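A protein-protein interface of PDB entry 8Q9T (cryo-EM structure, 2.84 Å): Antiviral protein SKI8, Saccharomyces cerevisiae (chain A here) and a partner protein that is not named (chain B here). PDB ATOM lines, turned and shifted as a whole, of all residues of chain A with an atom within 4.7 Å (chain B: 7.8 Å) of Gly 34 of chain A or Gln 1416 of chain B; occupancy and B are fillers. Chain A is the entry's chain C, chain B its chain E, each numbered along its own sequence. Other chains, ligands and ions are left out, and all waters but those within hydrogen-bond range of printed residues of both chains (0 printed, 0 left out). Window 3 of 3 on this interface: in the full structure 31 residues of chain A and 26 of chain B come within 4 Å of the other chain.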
ATOM      1  N   ALA A  17      -4.637  -5.161   9.459  1.00  0.00           N
ATOM      2  CA  ALA A  17      -4.947  -5.434   8.065  1.00  0.00           C
ATOM      3  C   ALA A  17      -5.860  -4.325   7.558  1.00  0.00           C
ATOM      4  O   ALA A  17      -6.020  -3.288   8.207  1.00  0.00           O
ATOM      5  CB  ALA A  17      -5.568  -6.827   7.909  1.00  0.00           C
ATOM      6  N   ASP A  18      -6.460  -4.542   6.393  1.00  0.00           N
ATOM      7  CA  ASP A  18      -7.290  -3.517   5.778  1.00  0.00           C
ATOM      8  C   ASP A  18      -8.547  -3.266   6.600  1.00  0.00           C
ATOM      9  O   ASP A  18      -9.211  -4.202   7.051  1.00  0.00           O
ATOM     10  CB  ASP A  18      -7.666  -3.926   4.356  1.00  0.00           C
ATOM     11  CG  ASP A  18      -6.510  -3.796   3.388  1.00  0.00           C
ATOM     12  OD1 ASP A  18      -5.691  -2.869   3.556  1.00  0.00           O
ATOM     13  OD2 ASP A  18      -6.417  -4.619   2.456  1.00  0.00           O
ATOM     14  N   PHE A  20     -12.099  -2.425   6.405  1.00  0.00           N
ATOM     15  CA  PHE A  20     -13.038  -2.554   5.300  1.00  0.00           C
ATOM     16  C   PHE A  20     -14.330  -1.771   5.492  1.00  0.00           C
ATOM     17  O   PHE A  20     -14.970  -1.410   4.499  1.00  0.00           O
ATOM     18  CB  PHE A  20     -13.371  -4.029   5.074  1.00  0.00           C
ATOM     19  CG  PHE A  20     -12.247  -4.820   4.471  1.00  0.00           C
ATOM     20  CD1 PHE A  20     -11.719  -4.473   3.243  1.00  0.00           C
ATOM     21  CD2 PHE A  20     -11.722  -5.915   5.132  1.00  0.00           C
ATOM     22  CE1 PHE A  20     -10.687  -5.203   2.688  1.00  0.00           C
ATOM     23  CE2 PHE A  20     -10.693  -6.645   4.582  1.00  0.00           C
ATOM     24  CZ  PHE A  20     -10.174  -6.288   3.359  1.00  0.00           C
ATOM     25  N   SER A  33     -11.971  -5.063  10.571  1.00  0.00           N
ATOM     26  CA  SER A  33     -10.772  -5.223   9.763  1.00  0.00           C
ATOM     27  C   SER A  33     -10.561  -6.691   9.434  1.00  0.00           C
ATOM     28  O   SER A  33     -11.243  -7.575   9.955  1.00  0.00           O
ATOM     29  CB  SER A  33      -9.542  -4.661  10.471  1.00  0.00           C
ATOM     30  OG  SER A  33      -8.379  -4.857   9.689  1.00  0.00           O
ATOM     31  N   GLY A  34      -9.592  -6.937   8.553  1.00  0.00           N
ATOM     32  CA  GLY A  34      -9.266  -8.280   8.120  1.00  0.00           C
ATOM     33  C   GLY A  34      -8.467  -9.101   9.103  1.00  0.00           C
ATOM     34  O   GLY A  34      -8.319 -10.308   8.898  1.00  0.00           O
ATOM     35  N   ASP A  35      -7.942  -8.484  10.162  1.00  0.00           N
ATOM     36  CA  ASP A  35      -7.267  -9.253  11.197  1.00  0.00           C
ATOM     37  C   ASP A  35      -8.241 -10.012  12.086  1.00  0.00           C
ATOM     38  O   ASP A  35      -7.817 -10.913  12.816  1.00  0.00           O
ATOM     39  CB  ASP A  35      -6.384  -8.340  12.054  1.00  0.00           C
ATOM     40  CG  ASP A  35      -7.105  -7.095  12.521  1.00  0.00           C
ATOM     41  OD1 ASP A  35      -8.347  -7.058  12.456  1.00  0.00           O
ATOM     42  OD2 ASP A  35      -6.426  -6.150  12.966  1.00  0.00           O
ATOM     43  N   GLY A  36      -9.525  -9.675  12.038  1.00  0.00           N
ATOM     44  CA  GLY A  36     -10.529 -10.361  12.815  1.00  0.00           C
ATOM     45  C   GLY A  36     -10.943  -9.686  14.100  1.00  0.00           C
ATOM     46  O   GLY A  36     -11.661 -10.301  14.894  1.00  0.00           O
ATOM     47  N   SER A  63     -10.926 -15.441  10.388  1.00  0.00           N
ATOM     48  CA  SER A  63     -10.970 -15.182   8.954  1.00  0.00           C
ATOM     49  C   SER A  63     -10.900 -13.696   8.625  1.00  0.00           C
ATOM     50  O   SER A  63     -10.319 -13.321   7.602  1.00  0.00           O
ATOM     51  CB  SER A  63     -12.239 -15.789   8.357  1.00  0.00           C
ATOM     52  OG  SER A  63     -12.139 -15.885   6.950  1.00  0.00           O
ATOM     53  N   GLY A  64     -11.472 -12.846   9.464  1.00  0.00           N
ATOM     54  CA  GLY A  64     -11.540 -11.425   9.207  1.00  0.00           C
ATOM     55  C   GLY A  64     -12.974 -10.959   9.008  1.00  0.00           C
ATOM     56  O   GLY A  64     -13.890 -11.744   8.763  1.00  0.00           O
ATOM     57  N   LEU A  65     -13.161  -9.648   9.116  1.00  0.00           N
ATOM     58  CA  LEU A  65     -14.473  -9.032   9.017  1.00  0.00           C
ATOM     59  C   LEU A  65     -14.457  -7.968   7.928  1.00  0.00           C
ATOM     60  O   LEU A  65     -13.434  -7.318   7.697  1.00  0.00           O
ATOM     61  CB  LEU A  65     -14.886  -8.400  10.350  1.00  0.00           C
ATOM     62  CG  LEU A  65     -14.736  -9.251  11.612  1.00  0.00           C
ATOM     63  CD1 LEU A  65     -15.026  -8.411  12.837  1.00  0.00           C
ATOM     64  CD2 LEU A  65     -15.640 -10.465  11.569  1.00  0.00           C
ATOM     65  N   PHE A  89     -15.374 -13.067   6.714  1.00  0.00           N
ATOM     66  CA  PHE A  89     -14.987 -13.527   5.383  1.00  0.00           C
ATOM     67  C   PHE A  89     -15.439 -14.952   5.100  1.00  0.00           C
ATOM     68  O   PHE A  89     -15.611 -15.308   3.931  1.00  0.00           O
ATOM     69  CB  PHE A  89     -13.472 -13.419   5.200  1.00  0.00           C
ATOM     70  CG  PHE A  89     -13.023 -12.113   4.609  1.00  0.00           C
ATOM     71  CD1 PHE A  89     -13.006 -11.927   3.238  1.00  0.00           C
ATOM     72  CD2 PHE A  89     -12.621 -11.070   5.422  1.00  0.00           C
ATOM     73  CE1 PHE A  89     -12.598 -10.727   2.694  1.00  0.00           C
ATOM     74  CE2 PHE A  89     -12.211  -9.871   4.883  1.00  0.00           C
ATOM     75  CZ  PHE A  89     -12.201  -9.700   3.517  1.00  0.00           C
ATOM     76  N   TYR B1406      -3.732  -8.731  -7.251  1.00  0.00           N
ATOM     77  CA  TYR B1406      -3.567  -8.720  -5.801  1.00  0.00           C
ATOM     78  C   TYR B1406      -3.469 -10.133  -5.242  1.00  0.00           C
ATOM     79  O   TYR B1406      -2.630 -10.410  -4.378  1.00  0.00           O
ATOM     80  CB  TYR B1406      -4.723  -7.966  -5.146  1.00  0.00           C
ATOM     81  CG  TYR B1406      -4.527  -6.472  -5.098  1.00  0.00           C
ATOM     82  CD1 TYR B1406      -3.328  -5.926  -4.673  1.00  0.00           C
ATOM     83  CD2 TYR B1406      -5.542  -5.607  -5.478  1.00  0.00           C
ATOM     84  CE1 TYR B1406      -3.141  -4.563  -4.629  1.00  0.00           C
ATOM     85  CE2 TYR B1406      -5.366  -4.241  -5.436  1.00  0.00           C
ATOM     86  CZ  TYR B1406      -4.163  -3.724  -5.011  1.00  0.00           C
ATOM     87  OH  TYR B1406      -3.979  -2.363  -4.965  1.00  0.00           O
ATOM     88  N   CYS B1407      -4.315 -11.045  -5.723  1.00  0.00           N
ATOM     89  CA  CYS B1407      -4.300 -12.410  -5.218  1.00  0.00           C
ATOM     90  C   CYS B1407      -3.056 -13.182  -5.632  1.00  0.00           C
ATOM     91  O   CYS B1407      -2.698 -14.150  -4.954  1.00  0.00           O
ATOM     92  CB  CYS B1407      -5.547 -13.158  -5.684  1.00  0.00           C
ATOM     93  SG  CYS B1407      -7.074 -12.551  -4.954  1.00  0.00           S
ATOM     94  N   ASN B1411       0.109 -13.297  -0.338  1.00  0.00           N
ATOM     95  CA  ASN B1411      -0.053 -12.780   1.011  1.00  0.00           C
ATOM     96  C   ASN B1411      -1.513 -12.865   1.440  1.00  0.00           C
ATOM     97  O   ASN B1411      -2.425 -12.851   0.610  1.00  0.00           O
ATOM     98  CB  ASN B1411       0.432 -11.331   1.076  1.00  0.00           C
ATOM     99  CG  ASN B1411       0.647 -10.849   2.489  1.00  0.00           C
ATOM    100  OD1 ASN B1411       0.589 -11.626   3.439  1.00  0.00           O
ATOM    101  ND2 ASN B1411       0.898  -9.555   2.638  1.00  0.00           N
ATOM    102  N   LEU B1412      -1.733 -12.955   2.754  1.00  0.00           N
ATOM    103  CA  LEU B1412      -3.101 -13.011   3.264  1.00  0.00           C
ATOM    104  C   LEU B1412      -3.811 -11.672   3.104  1.00  0.00           C
ATOM    105  O   LEU B1412      -4.983 -11.630   2.710  1.00  0.00           O
ATOM    106  CB  LEU B1412      -3.105 -13.448   4.728  1.00  0.00           C
ATOM    107  CG  LEU B1412      -4.459 -13.416   5.441  1.00  0.00           C
ATOM    108  CD1 LEU B1412      -5.464 -14.332   4.761  1.00  0.00           C
ATOM    109  CD2 LEU B1412      -4.308 -13.781   6.906  1.00  0.00           C
ATOM    110  N   ARG B1413      -3.120 -10.568   3.404  1.00  0.00           N
ATOM    111  CA  ARG B1413      -3.726  -9.249   3.250  1.00  0.00           C
ATOM    112  C   ARG B1413      -4.107  -8.984   1.801  1.00  0.00           C
ATOM    113  O   ARG B1413      -5.197  -8.470   1.516  1.00  0.00           O
ATOM    114  CB  ARG B1413      -2.767  -8.166   3.740  1.00  0.00           C
ATOM    115  CG  ARG B1413      -2.317  -8.301   5.177  1.00  0.00           C
ATOM    116  CD  ARG B1413      -1.197  -7.319   5.461  1.00  0.00           C
ATOM    117  NE  ARG B1413      -1.006  -7.079   6.885  1.00  0.00           N
ATOM    118  CZ  ARG B1413       0.124  -7.311   7.538  1.00  0.00           C
ATOM    119  NH1 ARG B1413       1.188  -7.802   6.924  1.00  0.00           N
ATOM    120  NH2 ARG B1413       0.189  -7.043   8.837  1.00  0.00           N
ATOM    121  N   SER B1414      -3.218  -9.329   0.869  1.00  0.00           N
ATOM    122  CA  SER B1414      -3.492  -9.101  -0.544  1.00  0.00           C
ATOM    123  C   SER B1414      -4.641  -9.971  -1.033  1.00  0.00           C
ATOM    124  O   SER B1414      -5.470  -9.520  -1.831  1.00  0.00           O
ATOM    125  CB  SER B1414      -2.231  -9.360  -1.362  1.00  0.00           C
ATOM    126  OG  SER B1414      -1.269  -8.348  -1.136  1.00  0.00           O
ATOM    127  N   ILE B1415      -4.706 -11.221  -0.573  1.00  0.00           N
ATOM    128  CA  ILE B1415      -5.804 -12.099  -0.962  1.00  0.00           C
ATOM    129  C   ILE B1415      -7.127 -11.565  -0.431  1.00  0.00           C
ATOM    130  O   ILE B1415      -8.147 -11.584  -1.131  1.00  0.00           O
ATOM    131  CB  ILE B1415      -5.534 -13.537  -0.483  1.00  0.00           C
ATOM    132  CG1 ILE B1415      -4.458 -14.186  -1.351  1.00  0.00           C
ATOM    133  CG2 ILE B1415      -6.803 -14.365  -0.523  1.00  0.00           C
ATOM    134  CD1 ILE B1415      -3.987 -15.517  -0.838  1.00  0.00           C
ATOM    135  N   GLN B1416      -7.132 -11.074   0.810  1.00  0.00           N
ATOM    136  CA  GLN B1416      -8.350 -10.486   1.359  1.00  0.00           C
ATOM    137  C   GLN B1416      -8.777  -9.256   0.569  1.00  0.00           C
ATOM    138  O   GLN B1416      -9.964  -9.078   0.281  1.00  0.00           O
ATOM    139  CB  GLN B1416      -8.148 -10.133   2.831  1.00  0.00           C
ATOM    140  CG  GLN B1416      -8.469 -11.256   3.792  1.00  0.00           C
ATOM    141  CD  GLN B1416      -8.250 -10.857   5.232  1.00  0.00           C
ATOM    142  OE1 GLN B1416      -7.746  -9.773   5.514  1.00  0.00           O
ATOM    143  NE2 GLN B1416      -8.629 -11.730   6.153  1.00  0.00           N
ATOM    144  N   ARG B1417      -7.823  -8.395   0.208  1.00  0.00           N
ATOM    145  CA  ARG B1417      -8.154  -7.210  -0.580  1.00  0.00           C
ATOM    146  C   ARG B1417      -8.707  -7.587  -1.950  1.00  0.00           C
ATOM    147  O   ARG B1417      -9.692  -7.000  -2.419  1.00  0.00           O
ATOM    148  CB  ARG B1417      -6.918  -6.326  -0.725  1.00  0.00           C
ATOM    149  CG  ARG B1417      -7.190  -4.947  -1.283  1.00  0.00           C
ATOM    150  CD  ARG B1417      -5.896  -4.185  -1.478  1.00  0.00           C
ATOM    151  NE  ARG B1417      -5.125  -4.099  -0.245  1.00  0.00           N
ATOM    152  CZ  ARG B1417      -3.952  -4.686  -0.052  1.00  0.00           C
ATOM    153  NH1 ARG B1417      -3.375  -5.408  -0.998  1.00  0.00           N
ATOM    154  NH2 ARG B1417      -3.344  -4.550   1.124  1.00  0.00           N
ATOM    155  N   GLY B1418      -8.086  -8.568  -2.608  1.00  0.00           N
ATOM    156  CA  GLY B1418      -8.569  -8.997  -3.909  1.00  0.00           C
ATOM    157  C   GLY B1418      -9.942  -9.634  -3.847  1.00  0.00           C
ATOM    158  O   GLY B1418     -10.749  -9.475  -4.765  1.00  0.00           O
ATOM    159  N   MET B1419     -10.225 -10.377  -2.773  1.00  0.00           N
ATOM    160  CA  MET B1419     -11.558 -10.945  -2.608  1.00  0.00           C
ATOM    161  C   MET B1419     -12.588  -9.873  -2.280  1.00  0.00           C
ATOM    162  O   MET B1419     -13.752  -9.996  -2.670  1.00  0.00           O
ATOM    163  CB  MET B1419     -11.552 -12.018  -1.523  1.00  0.00           C
ATOM    164  CG  MET B1419     -12.792 -12.888  -1.532  1.00  0.00           C
ATOM    165  SD  MET B1419     -12.625 -14.362  -0.521  1.00  0.00           S
ATOM    166  CE  MET B1419     -14.326 -14.624  -0.037  1.00  0.00           C
ATOM    167  N   PHE B1420     -12.188  -8.829  -1.555  1.00  0.00           N
ATOM    168  CA  PHE B1420     -13.096  -7.712  -1.321  1.00  0.00           C
ATOM    169  C   PHE B1420     -13.440  -7.004  -2.624  1.00  0.00           C
ATOM    170  O   PHE B1420     -14.596  -6.627  -2.846  1.00  0.00           O
ATOM    171  CB  PHE B1420     -12.479  -6.732  -0.327  1.00  0.00           C
ATOM    172  CG  PHE B1420     -13.453  -5.738   0.227  1.00  0.00           C
ATOM    173  CD1 PHE B1420     -14.294  -6.079   1.268  1.00  0.00           C
ATOM    174  CD2 PHE B1420     -13.530  -4.460  -0.295  1.00  0.00           C
ATOM    175  CE1 PHE B1420     -15.190  -5.166   1.778  1.00  0.00           C
ATOM    176  CE2 PHE B1420     -14.425  -3.543   0.213  1.00  0.00           C
ATOM    177  CZ  PHE B1420     -15.254  -3.897   1.250  1.00  0.00           C
ATOM    178  N   LEU B1421     -12.450  -6.815  -3.499  1.00  0.00           N
ATOM    179  CA  LEU B1421     -12.706  -6.140  -4.767  1.00  0.00           C
ATOM    180  C   LEU B1421     -13.591  -6.954  -5.700  1.00  0.00           C
ATOM    181  O   LEU B1421     -14.229  -6.376  -6.585  1.00  0.00           O
ATOM    182  CB  LEU B1421     -11.391  -5.817  -5.475  1.00  0.00           C
ATOM    183  CG  LEU B1421     -10.697  -4.512  -5.086  1.00  0.00           C
ATOM    184  CD1 LEU B1421      -9.408  -4.353  -5.869  1.00  0.00           C
ATOM    185  CD2 LEU B1421     -11.610  -3.322  -5.307  1.00  0.00           C
ATOM    186  N   CYS B1422     -13.648  -8.272  -5.531  1.00  0.00           N
ATOM    187  CA  CYS B1422     -14.379  -9.122  -6.461  1.00  0.00           C
ATOM    188  C   CYS B1422     -14.728 -10.451  -5.802  1.00  0.00           C
ATOM    189  O   CYS B1422     -14.074 -11.467  -6.069  1.00  0.00           O
ATOM    190  CB  CYS B1422     -13.548  -9.348  -7.726  1.00  0.00           C
ATOM    191  SG  CYS B1422     -14.474  -9.870  -9.178  1.00  0.00           S
ATOM    192  N   ALA B1428      -9.806 -16.086  -6.075  1.00  0.00           N
ATOM    193  CA  ALA B1428      -9.630 -15.404  -4.795  1.00  0.00           C
ATOM    194  C   ALA B1428     -10.196 -16.226  -3.643  1.00  0.00           C
ATOM    195  O   ALA B1428      -9.558 -16.364  -2.592  1.00  0.00           O
ATOM    196  CB  ALA B1428     -10.290 -14.027  -4.842  1.00  0.00           C
ATOM    197  N   ALA B1431      -7.921 -19.225  -3.034  1.00  0.00           N
ATOM    198  CA  ALA B1431      -6.690 -18.846  -2.347  1.00  0.00           C
ATOM    199  C   ALA B1431      -6.942 -18.559  -0.872  1.00  0.00           C
ATOM    200  O   ALA B1431      -6.158 -18.979  -0.011  1.00  0.00           O
ATOM    201  CB  ALA B1431      -6.063 -17.634  -3.029  1.00  0.00           C
ATOM    202  N   LEU B1432      -8.028 -17.848  -0.559  1.00  0.00           N
ATOM    203  CA  LEU B1432      -8.342 -17.579   0.840  1.00  0.00           C
ATOM    204  C   LEU B1432      -8.607 -18.871   1.598  1.00  0.00           C
ATOM    205  O   LEU B1432      -8.187 -19.021   2.751  1.00  0.00           O
ATOM    206  CB  LEU B1432      -9.545 -16.645   0.952  1.00  0.00           C
ATOM    207  CG  LEU B1432      -9.879 -16.250   2.394  1.00  0.00           C
ATOM    208  CD1 LEU B1432      -8.740 -15.451   3.006  1.00  0.00           C
ATOM    209  CD2 LEU B1432     -11.180 -15.484   2.480  1.00  0.00           C
ATOM    210  N   CYS B1435      -5.364 -20.510   2.378  1.00  0.00           N
ATOM    211  CA  CYS B1435      -4.576 -19.868   3.428  1.00  0.00           C
ATOM    212  C   CYS B1435      -4.792 -20.542   4.777  1.00  0.00           C
ATOM    213  O   CYS B1435      -3.836 -20.773   5.524  1.00  0.00           O
ATOM    214  CB  CYS B1435      -4.918 -18.381   3.516  1.00  0.00           C
ATOM    215  SG  CYS B1435      -4.116 -17.353   2.273  1.00  0.00           S
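Among the printed residues, pairs that only touch across the chains: Phe 20 of chain A with Phe 1420 of chain B and Phe 89 of chain A with Gln 1416 of chain B.
The backbone carbonyl oxygen (O) of Gly 64 of chain A lies within hydrogen-bond range of the backbone NH (N) of Phe 89 of chain A, 2.9 Å away.
The backbone carbonyl oxygen of Asp 18 of chain A sits at hydrogen-bond distance from the side-chain hydroxyl of Ser 33 of chain A (2.8 Å).
O of Asp 18 of chain A sits at hydrogen-bond distance from N of Gly 34 of chain A.
Ala 17 of chain A touches none of the printed residues of chain B.
Printed residues of chain B within 4 Å of Asp 18 of chain A: Arg 1417 (3.0 Å).
No residue of chain B comes within 4 Å of Ser 33 of chain A.
Gly 34 of chain A touches one residue of chain B.
Of the printed residues of chain B, Ser 63 of chain A touches Gln 1416.
Gln 1416 of chain B touches just these residues of chain A: Gly 34 (3.1 Å), Ser 63 (2.7 Å) and Phe 89 (3.9 Å).
Ala 1431 of chain B touches none of the printed residues of chain A.
The nearest residue of chain B that does not touch Gly 34 of chain A is Leu 1412 of chain B (5.7 Å).
The nearest residue of chain A that does not touch Gln 1416 of chain B is Phe 20 of chain A (4.2 Å).
NE2 of Gln 1416 of chain B sits at hydrogen-bond distance from O of Gly 34 of chain A, 3.1 Å away.
The guanidinium group of Arg 1417 of chain B is in salt-bridge range of the side-chain carboxylate of Asp 18 of chain A, 3.0 Å away.
The side-chain amide nitrogen (NE2) of Gln 1416 of chain B lies within hydrogen-bond range of the backbone carbonyl oxygen (O) of Ser 63 of chain A, 2.7 Å away.
Of the 18 printed residues of chain B, 3 touch a printed residue of chain A.
Printed residues of chain B that touch a printed residue of chain A: Gln 1416, Arg 1417 and Phe 1420.
Hydrophobic or aromatic side chains of chain B within 4 Å of the printed part of chain A: Phe 1420.
Hydrophobic or aromatic side chains of chain A within 4 Å of the printed part of chain B: Phe 20 and Phe 89.
Among the printed residues, Asp or Glu carboxylates within 4 Å of a Lys or Arg side-chain nitrogen of the other chain: Asp 18 of chain A with Arg 1417 of chain B (3.0 Å).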
